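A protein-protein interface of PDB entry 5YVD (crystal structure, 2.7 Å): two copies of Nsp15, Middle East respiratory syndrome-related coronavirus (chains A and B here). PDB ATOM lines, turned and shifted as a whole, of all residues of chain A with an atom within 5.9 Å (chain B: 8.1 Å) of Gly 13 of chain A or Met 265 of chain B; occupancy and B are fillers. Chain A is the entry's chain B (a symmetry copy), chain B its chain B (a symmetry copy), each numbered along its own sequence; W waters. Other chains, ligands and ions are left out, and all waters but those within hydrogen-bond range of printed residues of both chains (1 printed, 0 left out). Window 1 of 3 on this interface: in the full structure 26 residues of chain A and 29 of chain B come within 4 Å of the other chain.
The backbone carbonyl oxygen (O) of Asn 8 of chain A is in hydrogen-bond range of the backbone NH (N) of Gly 13 of chain A (3.4 Å).
The backbone carbonyl oxygen (O) of Glu 263 of chain B lies within hydrogen-bond range of the backbone NH (N) of Phe 276 of chain B, at 3.0 Å.
O of Tyr 58 of chain A lies within hydrogen-bond range of NE of Arg 61 of chain A.
Printed residues of chain B within 4 Å of Val 9 of chain A: Met 265 (3.4 Å).
Of the printed residues of chain A, Glu 263 of chain B touches Tyr 58 and Arg 61.
Of chain A, only Val 9 (3.4 Å), Gly 13 (3.6 Å), Tyr 58 (3.1 Å) and Arg 61 (3.6 Å) come within 4 Å of Met 265 of chain B.
The nearest printed residue of chain A that does not touch Phe 276 of chain B is Gly 13 of chain A (4.04 Å).
Printed residues of chain B that touch a printed residue of chain A: Glu 263, Met 265, Leu 266, Lys 267, Phe 276, Ala 287 and Val 288.
Hydrophobic or aromatic side chains of chain B that line the printed part of chain A: Met 265, Leu 266, Phe 276, Ala 287 and Val 288.
Printed residues of chain A that touch a printed residue of chain B: Val 9, Val 10, Lys 11, Gln 12, Gly 13, His 14, Ile 40, Tyr 58 and Arg 61.
Hydrophobic or aromatic side chains of chain A within 4 Å of the printed part of chain B: Val 9, Val 10, His 14, Ile 40 and Tyr 58.
Among the printed residues, 16 pairs touch across the chains.
Among the printed residues, Asp or Glu carboxylates within 4 Å of a Lys or Arg side-chain nitrogen of the other chain: Arg 61 of chain A with Glu 263 of chain B (3.3 Å).
No position is printed for both chains.
Among the printed residues, merely in contact across the chains: Gln 12 of chain A with Val 288 of chain B (3.2 Å), Val 9 of chain A with Met 265 of chain B (3.4 Å), Gln 12 of chain A with Ala 287 of chain B (3.5 Å), Gly 13 of chain A with Val 288 of chain B (3.5 Å), Gly 13 of chain A with Met 265 of chain B (3.6 Å), Ile 40 of chain A with Leu 266 of chain B (3.6 Å), Lys 11 of chain A with Val 288 of chain B (3.6 Å), Arg 61 of chain A with Met 265 of chain B (3.6 Å), Val 10 of chain A with Leu 266 of chain B (3.6 Å), Gly 13 of chain A with Ala 287 of chain B (3.7 Å), His 14 of chain A with Ala 287 of chain B (3.7 Å), Arg 61 of chain A with Phe 276 of chain B (3.8 Å) and Ile 40 of chain A with Lys 267 of chain B (3.8 Å).
The guanidinium group (NH1) of Arg 61 of chain A lies within salt-bridge range of the side-chain carboxylate (OE1) of Glu 263 of chain B, 3.3 Å away.
The side-chain sulfur (SD) of Met 265 of chain B lies close to the side-chain hydroxyl (OH) of Tyr 58 of chain A, 3.7 Å away.
The side-chain carboxylate of Glu 263 of chain B sits at hydrogen-bond distance from the side-chain hydroxyl of Tyr 58 of chain A, 2.7 Å away.
Water W1 lies within hydrogen-bond range of O of Met 265 of chain B and O of Cys 41 of chain A.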
ATOM      1  N   ASN A   8     -31.545  19.498   7.965  1.00  0.00           N
ATOM      2  CA  ASN A   8     -30.169  20.043   8.025  1.00  0.00           C
ATOM      3  C   ASN A   8     -30.109  21.178   9.001  1.00  0.00           C
ATOM      4  O   ASN A   8     -29.210  21.223   9.820  1.00  0.00           O
ATOM      5  CB  ASN A   8     -29.693  20.604   6.676  1.00  0.00           C
ATOM      6  CG  ASN A   8     -28.971  19.583   5.833  1.00  0.00           C
ATOM      7  OD1 ASN A   8     -27.731  19.533   5.820  1.00  0.00           O
ATOM      8  ND2 ASN A   8     -29.734  18.761   5.111  1.00  0.00           N
ATOM      9  N   VAL A   9     -31.058  22.113   8.895  1.00  0.00           N
ATOM     10  CA  VAL A   9     -31.007  23.321   9.708  1.00  0.00           C
ATOM     11  C   VAL A   9     -31.109  22.969  11.195  1.00  0.00           C
ATOM     12  O   VAL A   9     -30.357  23.485  12.026  1.00  0.00           O
ATOM     13  CB  VAL A   9     -32.135  24.314   9.353  1.00  0.00           C
ATOM     14  CG1 VAL A   9     -32.189  25.448  10.382  1.00  0.00           C
ATOM     15  CG2 VAL A   9     -31.961  24.862   7.952  1.00  0.00           C
ATOM     16  N   VAL A  10     -32.038  22.083  11.528  1.00  0.00           N
ATOM     17  CA  VAL A  10     -32.212  21.650  12.916  1.00  0.00           C
ATOM     18  C   VAL A  10     -30.997  20.862  13.452  1.00  0.00           C
ATOM     19  O   VAL A  10     -30.564  21.064  14.588  1.00  0.00           O
ATOM     20  CB  VAL A  10     -33.473  20.780  13.057  1.00  0.00           C
ATOM     21  CG1 VAL A  10     -33.573  20.197  14.453  1.00  0.00           C
ATOM     22  CG2 VAL A  10     -34.716  21.598  12.742  1.00  0.00           C
ATOM     23  N   LYS A  11     -30.453  19.974  12.629  1.00  0.00           N
ATOM     24  CA  LYS A  11     -29.507  18.989  13.109  1.00  0.00           C
ATOM     25  C   LYS A  11     -28.093  19.511  13.083  1.00  0.00           C
ATOM     26  O   LYS A  11     -27.301  19.212  13.962  1.00  0.00           O
ATOM     27  CB  LYS A  11     -29.583  17.711  12.266  1.00  0.00           C
ATOM     28  CG  LYS A  11     -29.952  16.499  13.105  1.00  0.00           C
ATOM     29  CD  LYS A  11     -31.417  16.534  13.562  1.00  0.00           C
ATOM     30  CE  LYS A  11     -31.586  15.777  14.876  1.00  0.00           C
ATOM     31  NZ  LYS A  11     -32.930  15.202  15.083  1.00  0.00           N
ATOM     32  N   GLN A  12     -27.796  20.289  12.051  1.00  0.00           N
ATOM     33  CA  GLN A  12     -26.440  20.653  11.668  1.00  0.00           C
ATOM     34  C   GLN A  12     -26.253  22.199  11.631  1.00  0.00           C
ATOM     35  O   GLN A  12     -25.196  22.709  11.277  1.00  0.00           O
ATOM     36  CB  GLN A  12     -26.218  20.021  10.300  1.00  0.00           C
ATOM     37  CG  GLN A  12     -24.895  19.309  10.116  1.00  0.00           C
ATOM     38  CD  GLN A  12     -24.665  18.163  11.077  1.00  0.00           C
ATOM     39  OE1 GLN A  12     -25.227  17.098  10.918  1.00  0.00           O
ATOM     40  NE2 GLN A  12     -23.798  18.372  12.053  1.00  0.00           N
ATOM     41  N   GLY A  13     -27.284  22.937  12.023  1.00  0.00           N
ATOM     42  CA  GLY A  13     -27.217  24.388  12.096  1.00  0.00           C
ATOM     43  C   GLY A  13     -27.525  25.132  10.799  1.00  0.00           C
ATOM     44  O   GLY A  13     -27.910  26.296  10.850  1.00  0.00           O
ATOM     45  N   HIS A  14     -27.326  24.471   9.654  1.00  0.00           N
ATOM     46  CA  HIS A  14     -27.458  25.078   8.337  1.00  0.00           C
ATOM     47  C   HIS A  14     -27.350  23.977   7.316  1.00  0.00           C
ATOM     48  O   HIS A  14     -27.223  22.819   7.694  1.00  0.00           O
ATOM     49  CB  HIS A  14     -26.411  26.164   8.085  1.00  0.00           C
ATOM     50  CG  HIS A  14     -25.001  25.669   8.009  1.00  0.00           C
ATOM     51  ND1 HIS A  14     -24.198  25.874   6.905  1.00  0.00           N
ATOM     52  CD2 HIS A  14     -24.230  25.025   8.914  1.00  0.00           C
ATOM     53  CE1 HIS A  14     -23.007  25.354   7.123  1.00  0.00           C
ATOM     54  NE2 HIS A  14     -22.998  24.832   8.335  1.00  0.00           N
ATOM     55  N   PHE A  15     -27.415  24.311   6.033  1.00  0.00           N
ATOM     56  CA  PHE A  15     -27.388  23.269   5.023  1.00  0.00           C
ATOM     57  C   PHE A  15     -25.973  22.753   4.745  1.00  0.00           C
ATOM     58  O   PHE A  15     -25.051  23.509   4.424  1.00  0.00           O
ATOM     59  CB  PHE A  15     -28.078  23.686   3.726  1.00  0.00           C
ATOM     60  CG  PHE A  15     -28.181  22.568   2.736  1.00  0.00           C
ATOM     61  CD1 PHE A  15     -29.031  21.516   2.969  1.00  0.00           C
ATOM     62  CD2 PHE A  15     -27.408  22.550   1.594  1.00  0.00           C
ATOM     63  CE1 PHE A  15     -29.138  20.460   2.058  1.00  0.00           C
ATOM     64  CE2 PHE A  15     -27.492  21.499   0.683  1.00  0.00           C
ATOM     65  CZ  PHE A  15     -28.363  20.445   0.922  1.00  0.00           C
ATOM     66  N   ILE A  40     -43.087  24.478  15.657  1.00  0.00           N
ATOM     67  CA  ILE A  40     -42.066  25.464  16.015  1.00  0.00           C
ATOM     68  C   ILE A  40     -41.565  26.218  14.814  1.00  0.00           C
ATOM     69  O   ILE A  40     -41.158  25.622  13.812  1.00  0.00           O
ATOM     70  CB  ILE A  40     -40.885  24.811  16.755  1.00  0.00           C
ATOM     71  CG1 ILE A  40     -41.385  24.270  18.096  1.00  0.00           C
ATOM     72  CG2 ILE A  40     -39.759  25.822  16.944  1.00  0.00           C
ATOM     73  CD1 ILE A  40     -40.369  23.447  18.841  1.00  0.00           C
ATOM     74  N   CYS A  41     -41.583  27.537  14.953  1.00  0.00           N
ATOM     75  CA  CYS A  41     -41.288  28.466  13.872  1.00  0.00           C
ATOM     76  C   CYS A  41     -39.790  28.492  13.596  1.00  0.00           C
ATOM     77  O   CYS A  41     -39.007  28.878  14.454  1.00  0.00           O
ATOM     78  CB  CYS A  41     -41.792  29.872  14.245  1.00  0.00           C
ATOM     79  SG  CYS A  41     -41.790  31.028  12.863  1.00  0.00           S
ATOM     80  N   MET A  42     -39.400  28.069  12.401  1.00  0.00           N
ATOM     81  CA  MET A  42     -37.997  28.061  12.010  1.00  0.00           C
ATOM     82  C   MET A  42     -37.614  29.275  11.202  1.00  0.00           C
ATOM     83  O   MET A  42     -36.433  29.544  11.070  1.00  0.00           O
ATOM     84  CB  MET A  42     -37.706  26.864  11.132  1.00  0.00           C
ATOM     85  CG  MET A  42     -37.529  25.553  11.876  1.00  0.00           C
ATOM     86  SD  MET A  42     -36.877  24.273  10.767  1.00  0.00           S
ATOM     87  CE  MET A  42     -38.330  24.055   9.764  1.00  0.00           C
ATOM     88  N   TYR A  58     -31.420  31.030   2.783  1.00  0.00           N
ATOM     89  CA  TYR A  58     -30.926  31.241   4.106  1.00  0.00           C
ATOM     90  C   TYR A  58     -30.127  30.028   4.591  1.00  0.00           C
ATOM     91  O   TYR A  58     -28.921  30.123   4.865  1.00  0.00           O
ATOM     92  CB  TYR A  58     -32.103  31.510   5.026  1.00  0.00           C
ATOM     93  CG  TYR A  58     -31.747  31.497   6.481  1.00  0.00           C
ATOM     94  CD1 TYR A  58     -32.250  30.513   7.329  1.00  0.00           C
ATOM     95  CD2 TYR A  58     -30.891  32.459   7.011  1.00  0.00           C
ATOM     96  CE1 TYR A  58     -31.917  30.493   8.667  1.00  0.00           C
ATOM     97  CE2 TYR A  58     -30.567  32.453   8.354  1.00  0.00           C
ATOM     98  CZ  TYR A  58     -31.087  31.470   9.173  1.00  0.00           C
ATOM     99  OH  TYR A  58     -30.777  31.460  10.505  1.00  0.00           O
ATOM    100  N   ARG A  61     -26.848  29.952   3.347  1.00  0.00           N
ATOM    101  CA  ARG A  61     -25.904  31.036   3.533  1.00  0.00           C
ATOM    102  C   ARG A  61     -24.547  30.494   3.242  1.00  0.00           C
ATOM    103  O   ARG A  61     -24.330  29.356   3.453  1.00  0.00           O
ATOM    104  CB  ARG A  61     -25.897  31.227   5.034  1.00  0.00           C
ATOM    105  CG  ARG A  61     -26.648  32.385   5.611  1.00  0.00           C
ATOM    106  CD  ARG A  61     -26.793  32.170   7.099  1.00  0.00           C
ATOM    107  NE  ARG A  61     -27.467  30.919   7.336  1.00  0.00           N
ATOM    108  CZ  ARG A  61     -27.634  30.370   8.511  1.00  0.00           C
ATOM    109  NH1 ARG A  61     -27.191  30.952   9.582  1.00  0.00           N
ATOM    110  NH2 ARG A  61     -28.255  29.235   8.593  1.00  0.00           N
ATOM    111  N   MET B 262     -25.056  34.856  18.476  1.00  0.00           N
ATOM    112  CA  MET B 262     -25.631  33.509  18.466  1.00  0.00           C
ATOM    113  C   MET B 262     -26.936  33.528  17.708  1.00  0.00           C
ATOM    114  O   MET B 262     -27.682  34.469  17.839  1.00  0.00           O
ATOM    115  CB  MET B 262     -25.991  33.054  19.866  1.00  0.00           C
ATOM    116  CG  MET B 262     -25.043  33.463  20.967  1.00  0.00           C
ATOM    117  SD  MET B 262     -25.875  33.486  22.576  1.00  0.00           S
ATOM    118  CE  MET B 262     -26.630  31.880  22.586  1.00  0.00           C
ATOM    119  N   GLU B 263     -27.241  32.477  16.950  1.00  0.00           N
ATOM    120  CA  GLU B 263     -28.600  32.267  16.435  1.00  0.00           C
ATOM    121  C   GLU B 263     -29.109  30.980  17.067  1.00  0.00           C
ATOM    122  O   GLU B 263     -28.304  30.153  17.444  1.00  0.00           O
ATOM    123  CB  GLU B 263     -28.616  32.135  14.910  1.00  0.00           C
ATOM    124  CG  GLU B 263     -28.090  33.335  14.107  1.00  0.00           C
ATOM    125  CD  GLU B 263     -27.886  32.979  12.625  1.00  0.00           C
ATOM    126  OE1 GLU B 263     -26.713  32.926  12.145  1.00  0.00           O
ATOM    127  OE2 GLU B 263     -28.909  32.702  11.950  1.00  0.00           O
ATOM    128  N   GLU B 264     -30.422  30.810  17.224  1.00  0.00           N
ATOM    129  CA  GLU B 264     -30.958  29.518  17.659  1.00  0.00           C
ATOM    130  C   GLU B 264     -32.062  29.172  16.690  1.00  0.00           C
ATOM    131  O   GLU B 264     -33.038  29.912  16.550  1.00  0.00           O
ATOM    132  CB  GLU B 264     -31.434  29.525  19.118  1.00  0.00           C
ATOM    133  CG  GLU B 264     -31.930  28.161  19.636  1.00  0.00           C
ATOM    134  CD  GLU B 264     -32.314  28.122  21.146  1.00  0.00           C
ATOM    135  OE1 GLU B 264     -32.507  29.176  21.798  1.00  0.00           O
ATOM    136  OE2 GLU B 264     -32.455  27.006  21.685  1.00  0.00           O
ATOM    137  N   MET B 265     -31.876  28.057  15.993  1.00  0.00           N
ATOM    138  CA  MET B 265     -32.720  27.714  14.867  1.00  0.00           C
ATOM    139  C   MET B 265     -34.056  27.251  15.374  1.00  0.00           C
ATOM    140  O   MET B 265     -35.083  27.668  14.869  1.00  0.00           O
ATOM    141  CB  MET B 265     -32.075  26.624  14.033  1.00  0.00           C
ATOM    142  CG  MET B 265     -30.670  26.950  13.521  1.00  0.00           C
ATOM    143  SD  MET B 265     -30.392  28.607  12.846  1.00  0.00           S
ATOM    144  CE  MET B 265     -30.726  28.447  11.127  1.00  0.00           C
ATOM    145  N   LEU B 266     -34.012  26.423  16.418  1.00  0.00           N
ATOM    146  CA  LEU B 266     -35.185  25.793  17.028  1.00  0.00           C
ATOM    147  C   LEU B 266     -35.425  26.293  18.458  1.00  0.00           C
ATOM    148  O   LEU B 266     -35.056  25.661  19.431  1.00  0.00           O
ATOM    149  CB  LEU B 266     -34.982  24.273  17.027  1.00  0.00           C
ATOM    150  CG  LEU B 266     -36.224  23.398  16.900  1.00  0.00           C
ATOM    151  CD1 LEU B 266     -37.067  23.829  15.717  1.00  0.00           C
ATOM    152  CD2 LEU B 266     -35.810  21.954  16.734  1.00  0.00           C
ATOM    153  N   LYS B 267     -36.082  27.440  18.564  1.00  0.00           N
ATOM    154  CA  LYS B 267     -36.325  28.110  19.853  1.00  0.00           C
ATOM    155  C   LYS B 267     -37.348  27.424  20.777  1.00  0.00           C
ATOM    156  O   LYS B 267     -38.284  26.767  20.326  1.00  0.00           O
ATOM    157  CB  LYS B 267     -36.782  29.549  19.587  1.00  0.00           C
ATOM    158  CG  LYS B 267     -35.802  30.604  20.023  1.00  0.00           C
ATOM    159  CD  LYS B 267     -35.961  31.895  19.248  1.00  0.00           C
ATOM    160  CE  LYS B 267     -35.281  31.770  17.887  1.00  0.00           C
ATOM    161  NZ  LYS B 267     -34.528  32.996  17.523  1.00  0.00           N
ATOM    162  N   GLY B 268     -37.156  27.598  22.081  1.00  0.00           N
ATOM    163  CA  GLY B 268     -38.133  27.162  23.087  1.00  0.00           C
ATOM    164  C   GLY B 268     -37.523  26.324  24.189  1.00  0.00           C
ATOM    165  O   GLY B 268     -36.509  25.641  23.973  1.00  0.00           O
ATOM    166  N   ASN B 274     -29.190  24.321  21.153  1.00  0.00           N
ATOM    167  CA  ASN B 274     -28.119  24.373  20.174  1.00  0.00           C
ATOM    168  C   ASN B 274     -28.029  25.779  19.620  1.00  0.00           C
ATOM    169  O   ASN B 274     -29.044  26.393  19.323  1.00  0.00           O
ATOM    170  CB  ASN B 274     -28.385  23.387  19.046  1.00  0.00           C
ATOM    171  CG  ASN B 274     -28.279  21.937  19.498  1.00  0.00           C
ATOM    172  OD1 ASN B 274     -27.556  21.610  20.431  1.00  0.00           O
ATOM    173  ND2 ASN B 274     -28.972  21.060  18.810  1.00  0.00           N
ATOM    174  N   TYR B 275     -26.806  26.294  19.508  1.00  0.00           N
ATOM    175  CA  TYR B 275     -26.603  27.642  19.019  1.00  0.00           C
ATOM    176  C   TYR B 275     -25.655  27.618  17.861  1.00  0.00           C
ATOM    177  O   TYR B 275     -24.832  26.734  17.752  1.00  0.00           O
ATOM    178  CB  TYR B 275     -26.056  28.544  20.118  1.00  0.00           C
ATOM    179  CG  TYR B 275     -27.001  28.658  21.272  1.00  0.00           C
ATOM    180  CD1 TYR B 275     -26.821  27.897  22.412  1.00  0.00           C
ATOM    181  CD2 TYR B 275     -28.115  29.500  21.213  1.00  0.00           C
ATOM    182  CE1 TYR B 275     -27.705  27.986  23.482  1.00  0.00           C
ATOM    183  CE2 TYR B 275     -29.006  29.591  22.280  1.00  0.00           C
ATOM    184  CZ  TYR B 275     -28.789  28.836  23.412  1.00  0.00           C
ATOM    185  OH  TYR B 275     -29.650  28.898  24.467  1.00  0.00           O
ATOM    186  N   PHE B 276     -25.805  28.616  17.004  1.00  0.00           N
ATOM    187  CA  PHE B 276     -24.947  28.873  15.889  1.00  0.00           C
ATOM    188  C   PHE B 276     -24.128  30.088  16.334  1.00  0.00           C
ATOM    189  O   PHE B 276     -24.616  31.208  16.287  1.00  0.00           O
ATOM    190  CB  PHE B 276     -25.847  29.173  14.681  1.00  0.00           C
ATOM    191  CG  PHE B 276     -25.116  29.363  13.383  1.00  0.00           C
ATOM    192  CD1 PHE B 276     -24.832  28.275  12.565  1.00  0.00           C
ATOM    193  CD2 PHE B 276     -24.766  30.633  12.952  1.00  0.00           C
ATOM    194  CE1 PHE B 276     -24.192  28.441  11.356  1.00  0.00           C
ATOM    195  CE2 PHE B 276     -24.123  30.810  11.736  1.00  0.00           C
ATOM    196  CZ  PHE B 276     -23.835  29.710  10.939  1.00  0.00           C
ATOM    197  N   PHE B 285     -15.982  30.085  15.206  1.00  0.00           N
ATOM    198  CA  PHE B 285     -17.373  29.777  14.916  1.00  0.00           C
ATOM    199  C   PHE B 285     -17.708  28.264  14.978  1.00  0.00           C
ATOM    200  O   PHE B 285     -16.895  27.385  14.628  1.00  0.00           O
ATOM    201  CB  PHE B 285     -17.673  30.351  13.545  1.00  0.00           C
ATOM    202  CG  PHE B 285     -18.538  29.486  12.706  1.00  0.00           C
ATOM    203  CD1 PHE B 285     -19.899  29.562  12.824  1.00  0.00           C
ATOM    204  CD2 PHE B 285     -17.980  28.605  11.788  1.00  0.00           C
ATOM    205  CE1 PHE B 285     -20.714  28.768  12.052  1.00  0.00           C
ATOM    206  CE2 PHE B 285     -18.783  27.805  11.001  1.00  0.00           C
ATOM    207  CZ  PHE B 285     -20.155  27.883  11.139  1.00  0.00           C
ATOM    208  N   LYS B 286     -18.914  27.955  15.441  1.00  0.00           N
ATOM    209  CA  LYS B 286     -19.417  26.583  15.417  1.00  0.00           C
ATOM    210  C   LYS B 286     -20.907  26.590  15.045  1.00  0.00           C
ATOM    211  O   LYS B 286     -21.684  27.434  15.530  1.00  0.00           O
ATOM    212  CB  LYS B 286     -19.168  25.897  16.751  1.00  0.00           C
ATOM    213  CG  LYS B 286     -19.437  24.405  16.721  1.00  0.00           C
ATOM    214  CD  LYS B 286     -18.659  23.640  17.792  1.00  0.00           C
ATOM    215  CE  LYS B 286     -18.865  24.210  19.198  1.00  0.00           C
ATOM    216  NZ  LYS B 286     -18.150  23.407  20.234  1.00  0.00           N
ATOM    217  N   ALA B 287     -21.299  25.666  14.168  1.00  0.00           N
ATOM    218  CA  ALA B 287     -22.646  25.689  13.592  1.00  0.00           C
ATOM    219  C   ALA B 287     -23.672  25.126  14.564  1.00  0.00           C
ATOM    220  O   ALA B 287     -24.821  25.567  14.602  1.00  0.00           O
ATOM    221  CB  ALA B 287     -22.676  24.942  12.260  1.00  0.00           C
ATOM    222  N   VAL B 288     -23.236  24.156  15.355  1.00  0.00           N
ATOM    223  CA  VAL B 288     -24.062  23.520  16.391  1.00  0.00           C
ATOM    224  C   VAL B 288     -23.205  23.448  17.648  1.00  0.00           C
ATOM    225  O   VAL B 288     -22.398  22.550  17.794  1.00  0.00           O
ATOM    226  CB  VAL B 288     -24.501  22.065  16.002  1.00  0.00           C
ATOM    227  CG1 VAL B 288     -25.504  21.510  17.000  1.00  0.00           C
ATOM    228  CG2 VAL B 288     -25.100  22.008  14.613  1.00  0.00           C
ATOM    229  N   CYS B 289     -23.353  24.426  18.532  1.00  0.00           N
ATOM    230  CA  CYS B 289     -22.746  24.368  19.846  1.00  0.00           C
ATOM    231  C   CYS B 289     -23.855  23.984  20.812  1.00  0.00           C
ATOM    232  O   CYS B 289     -24.752  24.776  21.096  1.00  0.00           O
ATOM    233  CB  CYS B 289     -22.135  25.719  20.214  1.00  0.00           C
ATOM    234  SG  CYS B 289     -21.181  25.695  21.770  1.00  0.00           S
HETATM  235  O   HOH W   1     -36.239  30.247  15.117  1.00  0.00           O
